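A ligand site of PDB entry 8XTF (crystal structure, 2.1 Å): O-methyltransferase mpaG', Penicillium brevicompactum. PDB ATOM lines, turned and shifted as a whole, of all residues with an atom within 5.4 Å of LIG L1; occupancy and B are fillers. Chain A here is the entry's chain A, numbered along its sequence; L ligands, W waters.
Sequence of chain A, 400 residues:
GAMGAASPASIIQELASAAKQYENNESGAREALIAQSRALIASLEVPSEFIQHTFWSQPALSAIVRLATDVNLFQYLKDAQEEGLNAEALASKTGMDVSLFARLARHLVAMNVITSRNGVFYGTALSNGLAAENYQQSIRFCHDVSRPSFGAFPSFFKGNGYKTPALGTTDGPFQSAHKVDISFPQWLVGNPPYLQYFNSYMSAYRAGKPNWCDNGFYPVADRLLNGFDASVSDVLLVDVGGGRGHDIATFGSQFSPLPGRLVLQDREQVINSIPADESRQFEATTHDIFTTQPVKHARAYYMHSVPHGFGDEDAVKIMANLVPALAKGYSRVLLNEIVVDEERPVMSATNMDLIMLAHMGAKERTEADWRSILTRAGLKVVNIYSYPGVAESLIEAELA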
ATOM      1  N   PHE A 198      11.969 -10.119  22.463  1.00  0.00           N
ATOM      2  CA  PHE A 198      12.039  -8.845  21.752  1.00  0.00           C
ATOM      3  C   PHE A 198      11.793  -9.021  20.260  1.00  0.00           C
ATOM      4  O   PHE A 198      11.031  -8.267  19.656  1.00  0.00           O
ATOM      5  CB  PHE A 198      13.395  -8.182  21.996  1.00  0.00           C
ATOM      6  CG  PHE A 198      13.505  -6.809  21.401  1.00  0.00           C
ATOM      7  CD1 PHE A 198      13.057  -5.696  22.120  1.00  0.00           C
ATOM      8  CD2 PHE A 198      14.057  -6.612  20.137  1.00  0.00           C
ATOM      9  CE1 PHE A 198      13.161  -4.415  21.575  1.00  0.00           C
ATOM     10  CE2 PHE A 198      14.160  -5.331  19.592  1.00  0.00           C
ATOM     11  CZ  PHE A 198      13.711  -4.241  20.319  1.00  0.00           C
ATOM     12  N   ASN A 199      12.424 -10.045  19.665  1.00  0.00           N
ATOM     13  CA  ASN A 199      12.291 -10.240  18.221  1.00  0.00           C
ATOM     14  C   ASN A 199      10.861 -10.604  17.831  1.00  0.00           C
ATOM     15  O   ASN A 199      10.393 -10.200  16.761  1.00  0.00           O
ATOM     16  CB  ASN A 199      13.281 -11.310  17.742  1.00  0.00           C
ATOM     17  CG  ASN A 199      14.748 -10.871  17.846  1.00  0.00           C
ATOM     18  OD1 ASN A 199      15.073  -9.687  17.816  1.00  0.00           O
ATOM     19  ND2 ASN A 199      15.638 -11.846  17.975  1.00  0.00           N
ATOM     20  N   MET A 202       8.735  -7.388  17.919  1.00  0.00           N
ATOM     21  CA  MET A 202       8.818  -6.440  16.804  1.00  0.00           C
ATOM     22  C   MET A 202       7.762  -6.680  15.733  1.00  0.00           C
ATOM     23  O   MET A 202       7.391  -5.752  15.021  1.00  0.00           O
ATOM     24  CB  MET A 202      10.213  -6.465  16.179  1.00  0.00           C
ATOM     25  CG  MET A 202      11.295  -5.917  17.111  1.00  0.00           C
ATOM     26  SD  MET A 202      10.925  -4.277  17.787  1.00  0.00           S
ATOM     27  CE  MET A 202      10.322  -4.699  19.421  1.00  0.00           C
ATOM     28  N   SER A 203       7.251  -7.909  15.614  1.00  0.00           N
ATOM     29  CA  SER A 203       6.134  -8.172  14.722  1.00  0.00           C
ATOM     30  C   SER A 203       4.788  -7.839  15.350  1.00  0.00           C
ATOM     31  O   SER A 203       3.759  -7.925  14.668  1.00  0.00           O
ATOM     32  CB  SER A 203       6.150  -9.635  14.279  1.00  0.00           C
ATOM     33  OG  SER A 203       5.769 -10.526  15.327  1.00  0.00           O
ATOM     34  N   TYR A 205       4.302  -4.888  17.862  1.00  0.00           N
ATOM     35  CA  TYR A 205       4.107  -3.589  18.520  1.00  0.00           C
ATOM     36  C   TYR A 205       3.274  -2.614  17.675  1.00  0.00           C
ATOM     37  O   TYR A 205       2.630  -1.719  18.230  1.00  0.00           O
ATOM     38  CB  TYR A 205       5.438  -2.940  18.891  1.00  0.00           C
ATOM     39  CG  TYR A 205       6.216  -2.355  17.735  1.00  0.00           C
ATOM     40  CD1 TYR A 205       6.983  -3.166  16.925  1.00  0.00           C
ATOM     41  CD2 TYR A 205       6.203  -0.991  17.464  1.00  0.00           C
ATOM     42  CE1 TYR A 205       7.707  -2.669  15.856  1.00  0.00           C
ATOM     43  CE2 TYR A 205       6.934  -0.462  16.385  1.00  0.00           C
ATOM     44  CZ  TYR A 205       7.680  -1.308  15.585  1.00  0.00           C
ATOM     45  OH  TYR A 205       8.407  -0.843  14.491  1.00  0.00           O
ATOM     46  N   ASP A 239      15.829  -4.271   3.343  1.00  0.00           N
ATOM     47  CA  ASP A 239      15.302  -3.865   4.657  1.00  0.00           C
ATOM     48  C   ASP A 239      16.424  -3.943   5.698  1.00  0.00           C
ATOM     49  O   ASP A 239      16.765  -5.016   6.189  1.00  0.00           O
ATOM     50  CB  ASP A 239      14.117  -4.733   5.075  1.00  0.00           C
ATOM     51  CG  ASP A 239      13.421  -4.215   6.351  1.00  0.00           C
ATOM     52  OD1 ASP A 239      12.287  -4.685   6.668  1.00  0.00           O
ATOM     53  OD2 ASP A 239      13.983  -3.359   7.056  1.00  0.00           O
ATOM     54  N   GLY A 241      17.909  -3.737   9.134  1.00  0.00           N
ATOM     55  CA  GLY A 241      17.376  -3.882  10.479  1.00  0.00           C
ATOM     56  C   GLY A 241      15.945  -4.348  10.516  1.00  0.00           C
ATOM     57  O   GLY A 241      15.176  -3.914  11.384  1.00  0.00           O
ATOM     58  N   GLY A 242      15.540  -5.227   9.592  1.00  0.00           N
ATOM     59  CA  GLY A 242      14.145  -5.573   9.454  1.00  0.00           C
ATOM     60  C   GLY A 242      13.628  -6.695  10.353  1.00  0.00           C
ATOM     61  O   GLY A 242      12.562  -7.259  10.091  1.00  0.00           O
ATOM     62  N   GLY A 243      14.370  -7.023  11.395  1.00  0.00           N
ATOM     63  CA  GLY A 243      13.870  -8.022  12.326  1.00  0.00           C
ATOM     64  C   GLY A 243      13.820  -9.395  11.691  1.00  0.00           C
ATOM     65  O   GLY A 243      14.688  -9.777  10.916  1.00  0.00           O
ATOM     66  N   HIS A 246       9.085  -9.507   8.939  1.00  0.00           N
ATOM     67  CA  HIS A 246       7.653  -9.341   8.791  1.00  0.00           C
ATOM     68  C   HIS A 246       7.319  -8.182   7.834  1.00  0.00           C
ATOM     69  O   HIS A 246       6.398  -8.291   7.028  1.00  0.00           O
ATOM     70  CB  HIS A 246       7.020  -9.123  10.172  1.00  0.00           C
ATOM     71  CG  HIS A 246       7.821  -8.243  11.086  1.00  0.00           C
ATOM     72  ND1 HIS A 246       8.843  -8.721  11.891  1.00  0.00           N
ATOM     73  CD2 HIS A 246       7.768  -6.902  11.313  1.00  0.00           C
ATOM     74  CE1 HIS A 246       9.381  -7.719  12.569  1.00  0.00           C
ATOM     75  NE2 HIS A 246       8.749  -6.601  12.227  1.00  0.00           N
ATOM     76  N   ASP A 247       8.062  -7.072   7.907  1.00  0.00           N
ATOM     77  CA  ASP A 247       7.808  -5.945   7.001  1.00  0.00           C
ATOM     78  C   ASP A 247       8.172  -6.296   5.564  1.00  0.00           C
ATOM     79  O   ASP A 247       7.426  -5.977   4.638  1.00  0.00           O
ATOM     80  CB  ASP A 247       8.579  -4.703   7.427  1.00  0.00           C
ATOM     81  CG  ASP A 247       8.029  -4.044   8.704  1.00  0.00           C
ATOM     82  OD1 ASP A 247       6.795  -4.143   8.980  1.00  0.00           O
ATOM     83  OD2 ASP A 247       8.847  -3.432   9.422  1.00  0.00           O
ATOM     84  N   GLN A 265      18.267  -7.519   6.196  1.00  0.00           N
ATOM     85  CA  GLN A 265      19.517  -7.391   6.931  1.00  0.00           C
ATOM     86  C   GLN A 265      19.244  -7.196   8.421  1.00  0.00           C
ATOM     87  O   GLN A 265      18.494  -6.287   8.797  1.00  0.00           O
ATOM     88  CB  GLN A 265      20.356  -6.223   6.383  1.00  0.00           C
ATOM     89  CG  GLN A 265      21.006  -6.507   5.011  1.00  0.00           C
ATOM     90  CD  GLN A 265      21.707  -5.300   4.390  1.00  0.00           C
ATOM     91  OE1 GLN A 265      21.518  -4.173   4.832  1.00  0.00           O
ATOM     92  NE2 GLN A 265      22.505  -5.542   3.363  1.00  0.00           N
ATOM     93  N   ASP A 266      19.841  -8.035   9.269  1.00  0.00           N
ATOM     94  CA  ASP A 266      19.759  -7.807  10.716  1.00  0.00           C
ATOM     95  C   ASP A 266      20.922  -8.535  11.399  1.00  0.00           C
ATOM     96  O   ASP A 266      21.863  -8.995  10.754  1.00  0.00           O
ATOM     97  CB  ASP A 266      18.410  -8.260  11.282  1.00  0.00           C
ATOM     98  CG  ASP A 266      17.955  -7.399  12.478  1.00  0.00           C
ATOM     99  OD1 ASP A 266      18.589  -7.468  13.561  1.00  0.00           O
ATOM    100  OD2 ASP A 266      16.983  -6.632  12.345  1.00  0.00           O
ATOM    101  N   ARG A 267      20.841  -8.640  12.731  1.00  0.00           N
ATOM    102  CA  ARG A 267      21.825  -9.353  13.526  1.00  0.00           C
ATOM    103  C   ARG A 267      21.733 -10.864  13.297  1.00  0.00           C
ATOM    104  O   ARG A 267      20.665 -11.414  13.010  1.00  0.00           O
ATOM    105  CB  ARG A 267      21.652  -9.042  15.010  1.00  0.00           C
ATOM    106  CG  ARG A 267      21.558  -7.560  15.293  1.00  0.00           C
ATOM    107  CD  ARG A 267      22.937  -6.937  15.280  1.00  0.00           C
ATOM    108  NE  ARG A 267      23.630  -7.252  16.527  1.00  0.00           N
ATOM    109  CZ  ARG A 267      24.902  -6.985  16.767  1.00  0.00           C
ATOM    110  NH1 ARG A 267      25.678  -6.410  15.863  1.00  0.00           N
ATOM    111  NH2 ARG A 267      25.407  -7.278  17.968  1.00  0.00           N
ATOM    112  N   GLN A 269      21.793 -13.252  15.452  1.00  0.00           N
ATOM    113  CA  GLN A 269      20.859 -13.944  16.332  1.00  0.00           C
ATOM    114  C   GLN A 269      19.406 -13.751  15.882  1.00  0.00           C
ATOM    115  O   GLN A 269      18.546 -14.587  16.203  1.00  0.00           O
ATOM    116  CB  GLN A 269      21.022 -13.482  17.781  1.00  0.00           C
ATOM    117  CG  GLN A 269      21.027 -11.969  17.969  1.00  0.00           C
ATOM    118  CD  GLN A 269      19.628 -11.382  18.115  1.00  0.00           C
ATOM    119  OE1 GLN A 269      18.619 -12.114  18.207  1.00  0.00           O
ATOM    120  NE2 GLN A 269      19.552 -10.057  18.132  1.00  0.00           N
ATOM    121  N   VAL A 270      19.108 -12.660  15.158  1.00  0.00           N
ATOM    122  CA  VAL A 270      17.782 -12.480  14.580  1.00  0.00           C
ATOM    123  C   VAL A 270      17.607 -13.368  13.350  1.00  0.00           C
ATOM    124  O   VAL A 270      16.599 -14.091  13.230  1.00  0.00           O
ATOM    125  CB  VAL A 270      17.535 -10.997  14.220  1.00  0.00           C
ATOM    126  CG1 VAL A 270      16.234 -10.852  13.463  1.00  0.00           C
ATOM    127  CG2 VAL A 270      17.501 -10.122  15.456  1.00  0.00           C
ATOM    128  N   HIS A 287      23.973  -8.408   8.755  1.00  0.00           N
ATOM    129  CA  HIS A 287      24.676  -7.163   8.467  1.00  0.00           C
ATOM    130  C   HIS A 287      24.674  -6.334   9.740  1.00  0.00           C
ATOM    131  O   HIS A 287      23.763  -6.451  10.558  1.00  0.00           O
ATOM    132  CB  HIS A 287      24.033  -6.418   7.280  1.00  0.00           C
ATOM    133  CG  HIS A 287      24.565  -5.046   7.064  1.00  0.00           C
ATOM    134  ND1 HIS A 287      25.883  -4.791   6.757  1.00  0.00           N
ATOM    135  CD2 HIS A 287      23.966  -3.828   7.146  1.00  0.00           C
ATOM    136  CE1 HIS A 287      26.068  -3.481   6.632  1.00  0.00           C
ATOM    137  NE2 HIS A 287      24.918  -2.883   6.866  1.00  0.00           N
ATOM    138  N   ASP A 288      25.720  -5.545   9.921  1.00  0.00           N
ATOM    139  CA  ASP A 288      25.850  -4.606  11.039  1.00  0.00           C
ATOM    140  C   ASP A 288      25.636  -3.184  10.511  1.00  0.00           C
ATOM    141  O   ASP A 288      26.418  -2.704   9.692  1.00  0.00           O
ATOM    142  CB  ASP A 288      27.244  -4.749  11.672  1.00  0.00           C
ATOM    143  CG  ASP A 288      27.412  -3.952  12.953  1.00  0.00           C
ATOM    144  OD1 ASP A 288      26.741  -2.895  13.142  1.00  0.00           O
ATOM    145  OD2 ASP A 288      28.246  -4.363  13.781  1.00  0.00           O
ATOM    146  N   ILE A 289      24.585  -2.509  10.993  1.00  0.00           N
ATOM    147  CA  ILE A 289      24.250  -1.162  10.509  1.00  0.00           C
ATOM    148  C   ILE A 289      25.364  -0.153  10.762  1.00  0.00           C
ATOM    149  O   ILE A 289      25.315   0.961  10.211  1.00  0.00           O
ATOM    150  CB  ILE A 289      22.941  -0.645  11.136  1.00  0.00           C
ATOM    151  CG1 ILE A 289      23.104  -0.468  12.658  1.00  0.00           C
ATOM    152  CG2 ILE A 289      21.766  -1.543  10.754  1.00  0.00           C
ATOM    153  CD1 ILE A 289      21.840   0.028  13.397  1.00  0.00           C
ATOM    154  N   PHE A 290      26.365  -0.498  11.567  1.00  0.00           N
ATOM    155  CA  PHE A 290      27.497   0.365  11.817  1.00  0.00           C
ATOM    156  C   PHE A 290      28.698   0.045  10.934  1.00  0.00           C
ATOM    157  O   PHE A 290      29.792   0.533  11.201  1.00  0.00           O
ATOM    158  CB  PHE A 290      27.873   0.305  13.308  1.00  0.00           C
ATOM    159  CG  PHE A 290      26.851   0.934  14.204  1.00  0.00           C
ATOM    160  CD1 PHE A 290      26.743   2.313  14.287  1.00  0.00           C
ATOM    161  CD2 PHE A 290      25.953   0.143  14.908  1.00  0.00           C
ATOM    162  CE1 PHE A 290      25.771   2.909  15.105  1.00  0.00           C
ATOM    163  CE2 PHE A 290      24.982   0.732  15.718  1.00  0.00           C
ATOM    164  CZ  PHE A 290      24.888   2.112  15.819  1.00  0.00           C
ATOM    165  N   HIS A 304      13.030   0.843   9.307  1.00  0.00           N
ATOM    166  CA  HIS A 304      11.831   1.063  10.103  1.00  0.00           C
ATOM    167  C   HIS A 304      12.218   0.967  11.574  1.00  0.00           C
ATOM    168  O   HIS A 304      12.734  -0.067  12.012  1.00  0.00           O
ATOM    169  CB  HIS A 304      10.772   0.031   9.750  1.00  0.00           C
ATOM    170  CG  HIS A 304       9.458   0.260  10.436  1.00  0.00           C
ATOM    171  ND1 HIS A 304       8.406  -0.632  10.356  1.00  0.00           N
ATOM    172  CD2 HIS A 304       9.017   1.289  11.190  1.00  0.00           C
ATOM    173  CE1 HIS A 304       7.388  -0.168  11.045  1.00  0.00           C
ATOM    174  NE2 HIS A 304       7.728   0.996  11.566  1.00  0.00           N
ATOM    175  N   SER A 305      11.991   2.042  12.335  1.00  0.00           N
ATOM    176  CA  SER A 305      12.286   2.044  13.776  1.00  0.00           C
ATOM    177  C   SER A 305      13.714   1.570  14.068  1.00  0.00           C
ATOM    178  O   SER A 305      13.921   0.662  14.893  1.00  0.00           O
ATOM    179  CB  SER A 305      11.313   1.166  14.562  1.00  0.00           C
ATOM    180  OG  SER A 305       9.960   1.513  14.347  1.00  0.00           O
ATOM    181  N   VAL A 306      14.687   2.136  13.379  1.00  0.00           N
ATOM    182  CA  VAL A 306      16.068   1.731  13.652  1.00  0.00           C
ATOM    183  C   VAL A 306      16.862   2.921  14.185  1.00  0.00           C
ATOM    184  O   VAL A 306      17.216   2.888  15.374  1.00  0.00           O
ATOM    185  CB  VAL A 306      16.710   1.077  12.411  1.00  0.00           C
ATOM    186  CG1 VAL A 306      18.230   0.902  12.591  1.00  0.00           C
ATOM    187  CG2 VAL A 306      16.017  -0.260  12.116  1.00  0.00           C
ATOM    188  N   PHE A 310      18.899   5.587  18.593  1.00  0.00           N
ATOM    189  CA  PHE A 310      20.293   5.971  18.698  1.00  0.00           C
ATOM    190  C   PHE A 310      20.404   7.489  18.803  1.00  0.00           C
ATOM    191  O   PHE A 310      19.601   8.225  18.230  1.00  0.00           O
ATOM    192  CB  PHE A 310      21.080   5.430  17.480  1.00  0.00           C
ATOM    193  CG  PHE A 310      21.136   3.935  17.443  1.00  0.00           C
ATOM    194  CD1 PHE A 310      22.124   3.252  18.132  1.00  0.00           C
ATOM    195  CD2 PHE A 310      20.165   3.204  16.771  1.00  0.00           C
ATOM    196  CE1 PHE A 310      22.170   1.869  18.144  1.00  0.00           C
ATOM    197  CE2 PHE A 310      20.207   1.811  16.763  1.00  0.00           C
ATOM    198  CZ  PHE A 310      21.212   1.145  17.456  1.00  0.00           C
HETATM  199  N1  LIG L   1      12.488  -3.052  11.600  1.00  0.00           N
HETATM  200  C1  LIG L   1      11.793  -3.911  12.571  1.00  0.00           C
HETATM  201  C2  LIG L   1      12.586  -4.041  13.876  1.00  0.00           C
HETATM  202  C3  LIG L   1      12.821  -2.711  14.588  1.00  0.00           C
HETATM  203  S1  LIG L   1      13.637  -2.928  16.193  1.00  0.00           S
HETATM  204  C4  LIG L   1      10.389  -3.395  12.914  1.00  0.00           C
HETATM  205  O1  LIG L   1       9.468  -4.186  13.204  1.00  0.00           O
HETATM  206  O2  LIG L   1      10.152  -2.175  12.922  1.00  0.00           O
HETATM  207  C5  LIG L   1      15.314  -2.497  15.672  1.00  0.00           C
HETATM  208  C6  LIG L   1      16.035  -3.574  14.863  1.00  0.00           C
HETATM  209  O3  LIG L   1      17.385  -3.156  14.627  1.00  0.00           O
HETATM  210  C7  LIG L   1      16.134  -4.926  15.555  1.00  0.00           C
HETATM  211  O4  LIG L   1      15.683  -5.910  14.656  1.00  0.00           O
HETATM  212  C8  LIG L   1      17.628  -5.101  15.837  1.00  0.00           C
HETATM  213  O5  LIG L   1      18.093  -6.435  15.831  1.00  0.00           O
HETATM  214  C9  LIG L   1      18.265  -4.255  14.752  1.00  0.00           C
HETATM  215  N2  LIG L   1      19.640  -3.837  15.066  1.00  0.00           N
HETATM  216  C10 LIG L   1      20.065  -3.202  16.195  1.00  0.00           C
HETATM  217  N3  LIG L   1      21.390  -2.989  16.103  1.00  0.00           N
HETATM  218  C11 LIG L   1      21.835  -3.494  14.933  1.00  0.00           C
HETATM  219  C12 LIG L   1      23.107  -3.559  14.337  1.00  0.00           C
HETATM  220  N4  LIG L   1      24.188  -3.060  14.944  1.00  0.00           N
HETATM  221  N5  LIG L   1      23.221  -4.132  13.090  1.00  0.00           N
HETATM  222  C13 LIG L   1      22.117  -4.651  12.467  1.00  0.00           C
HETATM  223  N6  LIG L   1      20.874  -4.585  13.058  1.00  0.00           N
HETATM  224  C14 LIG L   1      20.732  -4.012  14.269  1.00  0.00           C
HETATM  225  C1  LG2 L   2      17.885  -2.746  19.965  1.00  0.00           C
HETATM  226  C2  LG2 L   2      16.692   0.246  17.828  1.00  0.00           C
HETATM  227  C3  LG2 L   2      18.964  -5.008  19.627  1.00  0.00           C
HETATM  228  C4  LG2 L   2      17.753  -5.840  19.912  1.00  0.00           C
HETATM  229  C5  LG2 L   2      20.750  -6.796  20.056  1.00  0.00           C
HETATM  230  C6  LG2 L   2      13.367  -0.301  20.299  1.00  0.00           C
HETATM  231  C7  LG2 L   2      15.866  -0.844  19.913  1.00  0.00           C
HETATM  232  C8  LG2 L   2      16.742  -0.784  18.917  1.00  0.00           C
HETATM  233  C9  LG2 L   2      17.869  -1.776  18.802  1.00  0.00           C
HETATM  234  C10 LG2 L   2      19.018  -3.700  19.805  1.00  0.00           C
HETATM  235  C11 LG2 L   2      10.374  -0.741  17.952  1.00  0.00           C
HETATM  236  C12 LG2 L   2      20.162  -5.758  19.104  1.00  0.00           C
HETATM  237  C13 LG2 L   2      12.557  -0.328  19.154  1.00  0.00           C
HETATM  238  C14 LG2 L   2      21.986  -7.495  19.526  1.00  0.00           C
HETATM  239  C15 LG2 L   2      11.213  -0.708  19.209  1.00  0.00           C
HETATM  240  C16 LG2 L   2      10.689  -1.054  20.434  1.00  0.00           C
HETATM  241  C17 LG2 L   2      11.453  -1.021  21.574  1.00  0.00           C
HETATM  242  C18 LG2 L   2      12.798  -0.641  21.519  1.00  0.00           C
HETATM  243  C19 LG2 L   2       9.315  -1.490  20.814  1.00  0.00           C
HETATM  244  C20 LG2 L   2      10.621  -1.430  22.711  1.00  0.00           C
HETATM  245  C21 LG2 L   2      14.803   0.179  20.223  1.00  0.00           C
HETATM  246  O1  LG2 L   2      13.561  -0.601  22.625  1.00  0.00           O
HETATM  247  O2  LG2 L   2      13.086  -0.003  17.949  1.00  0.00           O
HETATM  248  O3  LG2 L   2       9.363  -1.632  22.255  1.00  0.00           O
HETATM  249  O4  LG2 L   2      10.875  -1.603  23.870  1.00  0.00           O
HETATM  250  O5  LG2 L   2      23.098  -6.958  19.757  1.00  0.00           O
HETATM  251  O6  LG2 L   2      21.846  -8.563  18.870  1.00  0.00           O
HETATM  252  O   HOH W   1       6.939  -3.502  12.060  1.00  0.00           O
HETATM  253  O   HOH W   2      17.366  -8.221  17.832  1.00  0.00           O
HETATM  254  O   HOH W   3      23.029  -2.169  18.532  1.00  0.00           O
HETATM  255  O   HOH W   4      11.371  -3.523   9.166  1.00  0.00           O
HETATM  256  O   HOH W   5      14.206  -1.793   9.229  1.00  0.00           O
HETATM  257  O   HOH W   6      14.104  -7.973  15.812  1.00  0.00           O
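O1 of LIG L1 lies close to O of Met 202 (3.2 Å).
A nitrogen (N5) of LIG L1 lies close to the backbone carbonyl oxygen (O) of His 287.
Merely in contact with LIG L1: Gly 242 (3.7 Å), Gly 243 (3.6 Å), Asp 247 (3.8 Å), Arg 267 (3.5 Å), Val 270 (3.8 Å), Phe 290 (3.7 Å) and Ser 305 (3.5 Å).
Hydrophobic or aromatic side chains within 4 Å of LIG L1: Met 202, Tyr 205, His 246, Val 270, Ile 289, Phe 290 and His 304.
16 residues have an atom within 4 Å of LIG L1: Met 202, Tyr 205, Gly 241, Gly 242, Gly 243, His 246, Asp 247, Asp 266, Arg 267, Val 270, His 287, Asp 288, Ile 289, Phe 290, His 304 and Ser 305.
Water W4 lies within hydrogen-bond range of OD2 of Asp 247 (2.5 Å), N1 of LIG L1 (2.7 Å) and OD1 of Asp 239 (2.9 Å).
Water W2 lies within hydrogen-bond range of the side-chain amide oxygen (OD1) of Asn 199 (2.7 Å), an oxygen (O5) of LIG L1 (2.8 Å) and the side-chain amide nitrogen (NE2) of Gln 269 (2.9 Å).
Water W6 bridges OD1 of Asn 199 (2.8 Å) and O4 of LIG L1 (2.8 Å).
Water W1 lies within hydrogen-bond range of an oxygen (O1) of LIG L1 (2.9 Å) and the side-chain carboxylate of Asp 247 (3.1 Å).
Water W5 lies within hydrogen-bond range of OD2 of Asp 239 (2.7 Å), N of His 304 (2.9 Å), O of Gly 241 (3.2 Å) and N1 of LIG L1 (3.2 Å).
A nitrogen (N1) of LIG L1 sits at hydrogen-bond distance from the backbone carbonyl oxygen (O) of His 304, at 3.0 Å.
A nitrogen (N5) of LIG L1 is in hydrogen-bond range of the backbone NH (N) of Ile 289, 3.0 Å away.
NE2 of Gln 269 lies within hydrogen-bond range of O6 of LG2 L2 (2.8 Å).
ND1 of His 304 lies within hydrogen-bond range of O2 of LIG L1 (3.5 Å).
The backbone carbonyl oxygen (O) of Gly 241 is in hydrogen-bond range of a nitrogen (N1) of LIG L1.
OD1 of Asp 288 is in hydrogen-bond range of N4 of LIG L1 (3.1 Å).
NH2 of Arg 267 lies within salt-bridge range of O5 of LG2 L2 (2.9 Å).
An oxygen (O2) of LG2 L2 sits at hydrogen-bond distance from the backbone carbonyl oxygen of Ser 305 (3.2 Å).
The side-chain hydroxyl of Tyr 205 lies within hydrogen-bond range of an oxygen (O2) of LIG L1.
OD1 of Asp 266 is in hydrogen-bond range of O5 of LIG L1.
A ring nitrogen (NE2) of His 246 lies within hydrogen-bond range of an oxygen (O1) of LIG L1 (2.7 Å).
A ring nitrogen (ND1) of His 304 sits at hydrogen-bond distance from the side-chain carboxylate (OD2) of Asp 247.
N of Gly 242 lies within hydrogen-bond range of O of Gln 265.
The backbone carbonyl oxygen of Met 202 lies within hydrogen-bond range of a ring nitrogen (NE2) of His 246, at 3.2 Å.
OD1 of Asp 288 lies within hydrogen-bond range of N of Phe 290.
OD2 of Asp 266 sits at hydrogen-bond distance from N of Gly 242.
OH of Tyr 205 is in hydrogen-bond range of OG of Ser 305, 2.8 Å away.
NH1 of Arg 267 is in salt-bridge range of OD2 of Asp 288, at 3.9 Å.
The backbone NH (N) of His 287 sits at hydrogen-bond distance from the backbone carbonyl oxygen (O) of Asp 266 (3.0 Å).
A sulfur (S1) of LIG L1 sits close to an oxygen (O2) of LG2 L2 (3.5 Å).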
